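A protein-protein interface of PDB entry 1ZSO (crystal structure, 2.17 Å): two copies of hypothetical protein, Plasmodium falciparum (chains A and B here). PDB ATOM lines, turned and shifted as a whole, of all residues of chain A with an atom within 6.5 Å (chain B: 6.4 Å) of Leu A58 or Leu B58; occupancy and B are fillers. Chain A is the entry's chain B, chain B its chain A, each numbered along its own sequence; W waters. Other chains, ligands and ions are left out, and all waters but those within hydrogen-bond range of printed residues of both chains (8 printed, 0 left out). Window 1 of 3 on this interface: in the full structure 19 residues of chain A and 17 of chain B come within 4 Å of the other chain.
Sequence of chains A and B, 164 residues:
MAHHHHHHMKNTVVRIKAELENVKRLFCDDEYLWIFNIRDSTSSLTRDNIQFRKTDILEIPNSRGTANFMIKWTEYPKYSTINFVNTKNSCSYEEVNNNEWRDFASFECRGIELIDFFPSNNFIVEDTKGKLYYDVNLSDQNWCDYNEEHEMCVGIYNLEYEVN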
ATOM      1  N   ARG A  53      21.068   7.302  16.865  1.00  0.00           N
ATOM      2  CA  ARG A  53      20.577   6.468  17.988  1.00  0.00           C
ATOM      3  C   ARG A  53      19.096   6.152  17.856  1.00  0.00           C
ATOM      4  O   ARG A  53      18.345   6.949  17.311  1.00  0.00           O
ATOM      5  CB  ARG A  53      20.767   7.189  19.314  1.00  0.00           C
ATOM      6  CG  ARG A  53      22.227   7.307  19.739  1.00  0.00           C
ATOM      7  CD  ARG A  53      22.514   8.699  20.250  1.00  0.00           C
ATOM      8  NE  ARG A  53      22.125   9.693  19.230  1.00  0.00           N
ATOM      9  CZ  ARG A  53      22.923  10.124  18.249  1.00  0.00           C
ATOM     10  NH1 ARG A  53      24.181   9.688  18.177  1.00  0.00           N
ATOM     11  NH2 ARG A  53      22.464  11.001  17.349  1.00  0.00           N
ATOM     12  N   THR A  55      16.827   6.488  19.799  1.00  0.00           N
ATOM     13  CA  THR A  55      16.011   7.413  20.571  1.00  0.00           C
ATOM     14  C   THR A  55      15.839   8.721  19.830  1.00  0.00           C
ATOM     15  O   THR A  55      15.033   9.552  20.258  1.00  0.00           O
ATOM     16  CB  THR A  55      16.674   7.755  21.935  1.00  0.00           C
ATOM     17  OG1 THR A  55      17.991   8.183  21.688  1.00  0.00           O
ATOM     18  CG2 THR A  55      16.732   6.522  22.884  1.00  0.00           C
ATOM     19  N   ASP A  56      16.595   8.906  18.741  1.00  0.00           N
ATOM     20  CA  ASP A  56      16.534  10.160  17.965  1.00  0.00           C
ATOM     21  C   ASP A  56      15.141  10.324  17.364  1.00  0.00           C
ATOM     22  O   ASP A  56      14.550   9.359  16.877  1.00  0.00           O
ATOM     23  CB  ASP A  56      17.604  10.202  16.863  1.00  0.00           C
ATOM     24  CG  ASP A  56      19.024  10.217  17.411  1.00  0.00           C
ATOM     25  OD1 ASP A  56      19.165  10.365  18.635  1.00  0.00           O
ATOM     26  OD2 ASP A  56      19.998  10.101  16.614  1.00  0.00           O
ATOM     27  N   ILE A  57      14.595  11.547  17.440  1.00  0.00           N
ATOM     28  CA  ILE A  57      13.211  11.821  16.982  1.00  0.00           C
ATOM     29  C   ILE A  57      13.217  12.889  15.905  1.00  0.00           C
ATOM     30  O   ILE A  57      13.389  14.062  16.207  1.00  0.00           O
ATOM     31  CB  ILE A  57      12.287  12.273  18.156  1.00  0.00           C
ATOM     32  CG1 ILE A  57      12.168  11.164  19.195  1.00  0.00           C
ATOM     33  CG2 ILE A  57      10.897  12.646  17.655  1.00  0.00           C
ATOM     34  CD1 ILE A  57      11.533  11.598  20.520  1.00  0.00           C
ATOM     35  N   LEU A  58      13.009  12.473  14.652  1.00  0.00           N
ATOM     36  CA  LEU A  58      12.931  13.382  13.506  1.00  0.00           C
ATOM     37  C   LEU A  58      11.548  13.313  12.887  1.00  0.00           C
ATOM     38  O   LEU A  58      11.104  12.240  12.455  1.00  0.00           O
ATOM     39  CB  LEU A  58      13.944  13.024  12.427  1.00  0.00           C
ATOM     40  CG  LEU A  58      15.364  12.599  12.794  1.00  0.00           C
ATOM     41  CD1 LEU A  58      16.243  12.488  11.541  1.00  0.00           C
ATOM     42  CD2 LEU A  58      16.044  13.530  13.761  1.00  0.00           C
ATOM     43  N   GLU A  59      10.872  14.460  12.839  1.00  0.00           N
ATOM     44  CA  GLU A  59       9.531  14.544  12.311  1.00  0.00           C
ATOM     45  C   GLU A  59       9.626  14.554  10.788  1.00  0.00           C
ATOM     46  O   GLU A  59      10.326  15.368  10.223  1.00  0.00           O
ATOM     47  CB  GLU A  59       8.855  15.806  12.822  1.00  0.00           C
ATOM     48  CG  GLU A  59       8.696  15.855  14.330  1.00  0.00           C
ATOM     49  CD  GLU A  59       7.468  15.069  14.855  1.00  0.00           C
ATOM     50  OE1 GLU A  59       6.576  14.669  14.043  1.00  0.00           O
ATOM     51  OE2 GLU A  59       7.398  14.866  16.101  1.00  0.00           O
ATOM     52  N   ILE A  60       8.934  13.617  10.148  1.00  0.00           N
ATOM     53  CA  ILE A  60       8.909  13.499   8.699  1.00  0.00           C
ATOM     54  C   ILE A  60       7.880  14.455   8.081  1.00  0.00           C
ATOM     55  O   ILE A  60       6.724  14.510   8.495  1.00  0.00           O
ATOM     56  CB  ILE A  60       8.592  12.060   8.258  1.00  0.00           C
ATOM     57  CG1 ILE A  60       9.538  11.087   8.936  1.00  0.00           C
ATOM     58  CG2 ILE A  60       8.661  11.908   6.667  1.00  0.00           C
ATOM     59  CD1 ILE A  60       9.090   9.649   8.856  1.00  0.00           C
ATOM     60  N   GLY A  65       4.367  10.432  11.083  1.00  0.00           N
ATOM     61  CA  GLY A  65       5.420   9.605  11.660  1.00  0.00           C
ATOM     62  C   GLY A  65       6.751  10.310  11.873  1.00  0.00           C
ATOM     63  O   GLY A  65       6.966  11.459  11.450  1.00  0.00           O
ATOM     64  N   THR A  66       7.634   9.603  12.562  1.00  0.00           N
ATOM     65  CA  THR A  66       8.953  10.116  12.910  1.00  0.00           C
ATOM     66  C   THR A  66      10.017   9.126  12.445  1.00  0.00           C
ATOM     67  O   THR A  66       9.693   8.002  12.172  1.00  0.00           O
ATOM     68  CB  THR A  66       9.055  10.318  14.425  1.00  0.00           C
ATOM     69  OG1 THR A  66       8.930   9.045  15.081  1.00  0.00           O
ATOM     70  CG2 THR A  66       7.960  11.246  14.912  1.00  0.00           C
ATOM     71  N   ALA A  67      11.283   9.556  12.374  1.00  0.00           N
ATOM     72  CA  ALA A  67      12.400   8.688  12.021  1.00  0.00           C
ATOM     73  C   ALA A  67      13.600   8.961  12.923  1.00  0.00           C
ATOM     74  O   ALA A  67      13.708  10.024  13.539  1.00  0.00           O
ATOM     75  CB  ALA A  67      12.808   8.867  10.576  1.00  0.00           C
ATOM     76  N   ASN A  68      14.486   7.971  12.991  1.00  0.00           N
ATOM     77  CA  ASN A  68      15.736   8.047  13.746  1.00  0.00           C
ATOM     78  C   ASN A  68      16.837   8.668  12.879  1.00  0.00           C
ATOM     79  O   ASN A  68      17.755   9.315  13.395  1.00  0.00           O
ATOM     80  CB  ASN A  68      16.228   6.645  14.136  1.00  0.00           C
ATOM     81  CG  ASN A  68      15.371   5.984  15.149  1.00  0.00           C
ATOM     82  OD1 ASN A  68      15.271   4.764  15.147  1.00  0.00           O
ATOM     83  ND2 ASN A  68      14.756   6.760  16.040  1.00  0.00           N
ATOM     84  N   PHE A  69      16.724   8.429  11.568  1.00  0.00           N
ATOM     85  CA  PHE A  69      17.585   9.040  10.556  1.00  0.00           C
ATOM     86  C   PHE A  69      16.809   9.397   9.297  1.00  0.00           C
ATOM     87  O   PHE A  69      15.967   8.624   8.832  1.00  0.00           O
ATOM     88  CB  PHE A  69      18.750   8.114  10.153  1.00  0.00           C
ATOM     89  CG  PHE A  69      19.712   8.752   9.180  1.00  0.00           C
ATOM     90  CD1 PHE A  69      20.718   9.591   9.628  1.00  0.00           C
ATOM     91  CD2 PHE A  69      19.582   8.559   7.813  1.00  0.00           C
ATOM     92  CE1 PHE A  69      21.629  10.221   8.693  1.00  0.00           C
ATOM     93  CE2 PHE A  69      20.459   9.160   6.924  1.00  0.00           C
ATOM     94  CZ  PHE A  69      21.491  10.013   7.378  1.00  0.00           C
ATOM     95  N   MET A  70      17.155  10.553   8.735  1.00  0.00           N
ATOM     96  CA  MET A  70      16.581  11.023   7.481  1.00  0.00           C
ATOM     97  C   MET A  70      17.606  11.687   6.536  1.00  0.00           C
ATOM     98  O   MET A  70      18.601  12.272   6.963  1.00  0.00           O
ATOM     99  CB  MET A  70      15.518  12.082   7.738  1.00  0.00           C
ATOM    100  CG  MET A  70      14.146  11.598   8.088  1.00  0.00           C
ATOM    101  SD  MET A  70      12.905  13.146   7.676  1.00  0.00           S
ATOM    102  CE  MET A  70      13.173  14.155   9.281  1.00  0.00           C
ATOM    103  N   ILE A  71      17.311  11.624   5.243  1.00  0.00           N
ATOM    104  CA  ILE A  71      18.121  12.277   4.257  1.00  0.00           C
ATOM    105  C   ILE A  71      17.232  12.648   3.076  1.00  0.00           C
ATOM    106  O   ILE A  71      16.333  11.905   2.707  1.00  0.00           O
ATOM    107  CB  ILE A  71      19.359  11.407   3.888  1.00  0.00           C
ATOM    108  CG1 ILE A  71      20.310  12.145   2.953  1.00  0.00           C
ATOM    109  CG2 ILE A  71      18.992  10.053   3.261  1.00  0.00           C
ATOM    110  CD1 ILE A  71      21.634  11.415   2.844  1.00  0.00           C
ATOM    111  N   GLN B  51      22.020  17.780   7.376  1.00  0.00           N
ATOM    112  CA  GLN B  51      20.648  18.192   7.198  1.00  0.00           C
ATOM    113  C   GLN B  51      19.945  18.053   8.515  1.00  0.00           C
ATOM    114  O   GLN B  51      20.043  17.004   9.156  1.00  0.00           O
ATOM    115  CB  GLN B  51      19.969  17.301   6.160  1.00  0.00           C
ATOM    116  CG  GLN B  51      20.525  17.520   4.732  1.00  0.00           C
ATOM    117  CD  GLN B  51      19.956  16.544   3.730  1.00  0.00           C
ATOM    118  OE1 GLN B  51      19.077  15.785   4.054  1.00  0.00           O
ATOM    119  NE2 GLN B  51      20.427  16.599   2.495  1.00  0.00           N
ATOM    120  N   ARG B  53      16.200  19.769  10.879  1.00  0.00           N
ATOM    121  CA  ARG B  53      15.203  20.744  11.242  1.00  0.00           C
ATOM    122  C   ARG B  53      15.377  21.146  12.676  1.00  0.00           C
ATOM    123  O   ARG B  53      15.921  20.383  13.473  1.00  0.00           O
ATOM    124  CB  ARG B  53      13.798  20.178  11.071  1.00  0.00           C
ATOM    125  CG  ARG B  53      13.607  19.714   9.702  1.00  0.00           C
ATOM    126  CD  ARG B  53      12.389  18.970   9.489  1.00  0.00           C
ATOM    127  NE  ARG B  53      12.252  18.831   8.049  1.00  0.00           N
ATOM    128  CZ  ARG B  53      12.952  17.961   7.338  1.00  0.00           C
ATOM    129  NH1 ARG B  53      13.864  17.167   7.942  1.00  0.00           N
ATOM    130  NH2 ARG B  53      12.764  17.899   6.034  1.00  0.00           N
ATOM    131  N   THR B  55      13.235  21.348  14.862  1.00  0.00           N
ATOM    132  CA  THR B  55      12.419  20.518  15.721  1.00  0.00           C
ATOM    133  C   THR B  55      13.034  19.135  16.032  1.00  0.00           C
ATOM    134  O   THR B  55      12.465  18.355  16.829  1.00  0.00           O
ATOM    135  CB  THR B  55      11.053  20.217  15.061  1.00  0.00           C
ATOM    136  OG1 THR B  55      11.259  19.683  13.746  1.00  0.00           O
ATOM    137  CG2 THR B  55      10.180  21.422  14.986  1.00  0.00           C
ATOM    138  N   ASP B  56      14.115  18.776  15.362  1.00  0.00           N
ATOM    139  CA  ASP B  56      14.813  17.489  15.647  1.00  0.00           C
ATOM    140  C   ASP B  56      15.255  17.400  17.112  1.00  0.00           C
ATOM    141  O   ASP B  56      15.741  18.350  17.677  1.00  0.00           O
ATOM    142  CB  ASP B  56      16.013  17.264  14.725  1.00  0.00           C
ATOM    143  CG  ASP B  56      15.596  17.062  13.251  1.00  0.00           C
ATOM    144  OD1 ASP B  56      14.422  16.725  13.038  1.00  0.00           O
ATOM    145  OD2 ASP B  56      16.433  17.209  12.319  1.00  0.00           O
ATOM    146  N   ILE B  57      15.061  16.256  17.718  1.00  0.00           N
ATOM    147  CA  ILE B  57      15.399  16.046  19.099  1.00  0.00           C
ATOM    148  C   ILE B  57      16.358  14.858  19.167  1.00  0.00           C
ATOM    149  O   ILE B  57      15.962  13.696  18.925  1.00  0.00           O
ATOM    150  CB  ILE B  57      14.126  15.679  19.931  1.00  0.00           C
ATOM    151  CG1 ILE B  57      13.083  16.819  19.922  1.00  0.00           C
ATOM    152  CG2 ILE B  57      14.506  15.282  21.344  1.00  0.00           C
ATOM    153  CD1 ILE B  57      11.724  16.343  20.405  1.00  0.00           C
ATOM    154  N   LEU B  58      17.612  15.175  19.462  1.00  0.00           N
ATOM    155  CA  LEU B  58      18.636  14.202  19.745  1.00  0.00           C
ATOM    156  C   LEU B  58      19.112  14.438  21.153  1.00  0.00           C
ATOM    157  O   LEU B  58      19.384  15.565  21.526  1.00  0.00           O
ATOM    158  CB  LEU B  58      19.823  14.394  18.806  1.00  0.00           C
ATOM    159  CG  LEU B  58      19.569  14.657  17.328  1.00  0.00           C
ATOM    160  CD1 LEU B  58      20.870  14.549  16.523  1.00  0.00           C
ATOM    161  CD2 LEU B  58      18.486  13.814  16.757  1.00  0.00           C
ATOM    162  N   GLU B  59      19.201  13.378  21.929  1.00  0.00           N
ATOM    163  CA  GLU B  59      19.601  13.467  23.316  1.00  0.00           C
ATOM    164  C   GLU B  59      21.106  13.555  23.435  1.00  0.00           C
ATOM    165  O   GLU B  59      21.819  12.710  22.908  1.00  0.00           O
ATOM    166  CB  GLU B  59      19.081  12.262  24.083  1.00  0.00           C
ATOM    167  CG  GLU B  59      17.561  12.254  24.185  1.00  0.00           C
ATOM    168  CD  GLU B  59      17.029  13.353  25.134  1.00  0.00           C
ATOM    169  OE1 GLU B  59      17.821  13.838  25.974  1.00  0.00           O
ATOM    170  OE2 GLU B  59      15.818  13.720  25.050  1.00  0.00           O
ATOM    171  N   ILE B  60      21.573  14.617  24.089  1.00  0.00           N
ATOM    172  CA  ILE B  60      23.005  14.833  24.307  1.00  0.00           C
ATOM    173  C   ILE B  60      23.423  14.113  25.573  1.00  0.00           C
ATOM    174  O   ILE B  60      22.817  14.300  26.606  1.00  0.00           O
ATOM    175  CB  ILE B  60      23.345  16.312  24.495  1.00  0.00           C
ATOM    176  CG1 ILE B  60      22.901  17.126  23.293  1.00  0.00           C
ATOM    177  CG2 ILE B  60      24.850  16.495  24.739  1.00  0.00           C
ATOM    178  CD1 ILE B  60      22.906  18.624  23.571  1.00  0.00           C
ATOM    179  N   GLY B  65      19.947  18.570  27.954  1.00  0.00           N
ATOM    180  CA  GLY B  65      19.656  19.237  26.705  1.00  0.00           C
ATOM    181  C   GLY B  65      19.539  18.295  25.520  1.00  0.00           C
ATOM    182  O   GLY B  65      20.029  17.156  25.546  1.00  0.00           O
ATOM    183  N   THR B  66      18.874  18.782  24.478  1.00  0.00           N
ATOM    184  CA  THR B  66      18.808  18.057  23.241  1.00  0.00           C
ATOM    185  C   THR B  66      19.405  18.954  22.150  1.00  0.00           C
ATOM    186  O   THR B  66      19.640  20.143  22.366  1.00  0.00           O
ATOM    187  CB  THR B  66      17.379  17.589  22.947  1.00  0.00           C
ATOM    188  OG1 THR B  66      16.543  18.724  22.738  1.00  0.00           O
ATOM    189  CG2 THR B  66      16.820  16.737  24.141  1.00  0.00           C
ATOM    190  N   ALA B  67      19.702  18.354  21.021  1.00  0.00           N
ATOM    191  CA  ALA B  67      20.366  19.018  19.948  1.00  0.00           C
ATOM    192  C   ALA B  67      19.552  18.702  18.718  1.00  0.00           C
ATOM    193  O   ALA B  67      18.826  17.709  18.719  1.00  0.00           O
ATOM    194  CB  ALA B  67      21.749  18.472  19.807  1.00  0.00           C
ATOM    195  N   ASN B  68      19.666  19.533  17.688  1.00  0.00           N
ATOM    196  CA  ASN B  68      19.002  19.277  16.395  1.00  0.00           C
ATOM    197  C   ASN B  68      19.931  18.483  15.515  1.00  0.00           C
ATOM    198  O   ASN B  68      19.509  17.845  14.555  1.00  0.00           O
ATOM    199  CB  ASN B  68      18.719  20.581  15.636  1.00  0.00           C
ATOM    200  CG  ASN B  68      17.819  21.492  16.375  1.00  0.00           C
ATOM    201  OD1 ASN B  68      17.981  22.729  16.328  1.00  0.00           O
ATOM    202  ND2 ASN B  68      16.846  20.909  17.080  1.00  0.00           N
ATOM    203  N   PHE B  69      21.230  18.633  15.774  1.00  0.00           N
ATOM    204  CA  PHE B  69      22.230  17.862  15.039  1.00  0.00           C
ATOM    205  C   PHE B  69      23.406  17.503  15.932  1.00  0.00           C
ATOM    206  O   PHE B  69      23.864  18.313  16.746  1.00  0.00           O
ATOM    207  CB  PHE B  69      22.727  18.618  13.801  1.00  0.00           C
ATOM    208  CG  PHE B  69      23.792  17.884  13.047  1.00  0.00           C
ATOM    209  CD1 PHE B  69      23.455  16.980  12.049  1.00  0.00           C
ATOM    210  CD2 PHE B  69      25.128  18.062  13.369  1.00  0.00           C
ATOM    211  CE1 PHE B  69      24.450  16.281  11.352  1.00  0.00           C
ATOM    212  CE2 PHE B  69      26.126  17.390  12.681  1.00  0.00           C
ATOM    213  CZ  PHE B  69      25.776  16.480  11.661  1.00  0.00           C
ATOM    214  N   MET B  70      23.862  16.268  15.807  1.00  0.00           N
ATOM    215  CA  MET B  70      25.128  15.907  16.401  1.00  0.00           C
ATOM    216  C   MET B  70      26.015  14.987  15.626  1.00  0.00           C
ATOM    217  O   MET B  70      25.601  14.257  14.739  1.00  0.00           O
ATOM    218  CB  MET B  70      24.997  15.361  17.819  1.00  0.00           C
ATOM    219  CG  MET B  70      23.817  14.593  18.224  1.00  0.00           C
ATOM    220  SD  MET B  70      24.040  14.335  20.266  1.00  0.00           S
ATOM    221  CE  MET B  70      25.710  14.921  20.489  1.00  0.00           C
HETATM  222  O   HOH W   1      18.064  15.050   8.797  1.00  0.00           O
HETATM  223  O   HOH W   2      18.260  10.779  20.984  1.00  0.00           O
HETATM  224  O   HOH W   3      17.129  15.149   6.124  1.00  0.00           O
HETATM  225  O   HOH W   4       9.463  17.793   9.663  1.00  0.00           O
HETATM  226  O   HOH W   5      11.466  15.966  16.593  1.00  0.00           O
HETATM  227  O   HOH W   6      26.078  11.494  16.344  1.00  0.00           O
HETATM  228  O   HOH W   7      11.878  17.008  13.751  1.00  0.00           O
HETATM  229  O   HOH W   8      23.521  11.872  14.725  1.00  0.00           O
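O of Ile B57 sits at hydrogen-bond distance from N of Ile A57, at 2.9 Å.
N of Arg B53 lies within hydrogen-bond range of OD2 of Asp B56 (2.9 Å). The side-chain amide nitrogen of Asn B68 sits at hydrogen-bond distance from the backbone carbonyl oxygen of Asp B56 (2.9 Å). O of Leu B58 is in hydrogen-bond range of N of Ala B67. OD2 of Asp A56 is in salt-bridge range of NH2 of Arg A53. ND2 of Asn A68 lies within hydrogen-bond range of O of Asp A56. O of Leu A58 lies within hydrogen-bond range of N of Ala A67 (2.7 Å).
Among the printed residues, merely in contact across the chains: Met A70 with Arg B53 (3.4 Å), Leu A58 with Asp B56 (3.6 Å), Ile A71 with Gln B51 (3.6 Å), Asp A56 with Leu B58 (3.7 Å), Asp A56 with Ile B57 (3.7 Å), Ile A57 with Asp B56 (3.8 Å), Leu A58 with Leu B58 (3.9 Å), Arg A53 with Met B70 (3.9 Å) and Arg A53 with Leu B58 (3.98 Å).
Of the 14 printed residues of chain A, 6 touch a printed residue of chain B. Hydrophobic or aromatic side chains of chain A that line the printed part of chain B: Leu A58, Met A70 and Ile A71. Of the 14 printed residues of chain B, 6 touch a printed residue of chain A. Printed residues of chain B that touch a printed residue of chain A: Gln B51, Arg B53, Asp B56, Ile B57, Leu B58 and Met B70. Hydrophobic or aromatic side chains of chain B within 4 Å of the printed part of chain A: Leu B58 and Met B70.
Printed residues of chain B within 4 Å of Leu A58: Asp B56 and Leu B58. Leu B58 touches three residues of chain A. Printed residues of chain B within 4 Å of Ile A57: Asp B56 (3.8 Å) and Ile B57 (2.9 Å). Printed residues of chain A within 4 Å of Met B70: Arg A53. Of the printed residues of chain B, Met A70 touches Arg B53. Printed residues of chain B within 4 Å of Arg A53: Leu B58 and Met B70. Of the printed residues of chain A, Gln B51 touches Ile A71 (3.6 Å). The nearest residue of chain B that does not touch Leu A58 is Ile B57 (4.9 Å). The nearest residue of chain A that does not touch Leu B58 is Ile A57 (4.6 Å).
Arg A53 touches Leu B58, but with the chains exchanged Leu A58 does not touch Arg B53 (6.1 Å). Asp A56 touches Leu B58, and with the chains exchanged Leu A58 touches Asp B56. Ile A57 touches its own counterpart, Ile B57. Leu B58 touches its own counterpart, Leu A58. Positions printed for both chains: 53, 55, 56, 57, 58, 59, 60, 65, 66, 67, 68, 69 and 70.
Water W2 lies within hydrogen-bond range of the side-chain carboxylate (OD1) of Asp A56 (2.6 Å), the side-chain hydroxyl (OG1) of Thr A55 (2.7 Å) and the backbone NH (N) of Glu B59 (2.9 Å). Water W4 lies within hydrogen-bond range of O of Glu A59 and NE of Arg B53. Water W1 bridges the backbone carbonyl oxygen of Gln B51 (2.8 Å) and the backbone carbonyl oxygen of Met A70 (3.4 Å). Water W3 lies within hydrogen-bond range of OE1 of Gln B51 and O of Met A70. Water W8 bridges the guanidinium group (NH2) of Arg A53 (3.0 Å) and the backbone carbonyl oxygen (O) of Met B70 (3.2 Å). Water W6 bridges NH1 of Arg A53 and O of Met B70.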
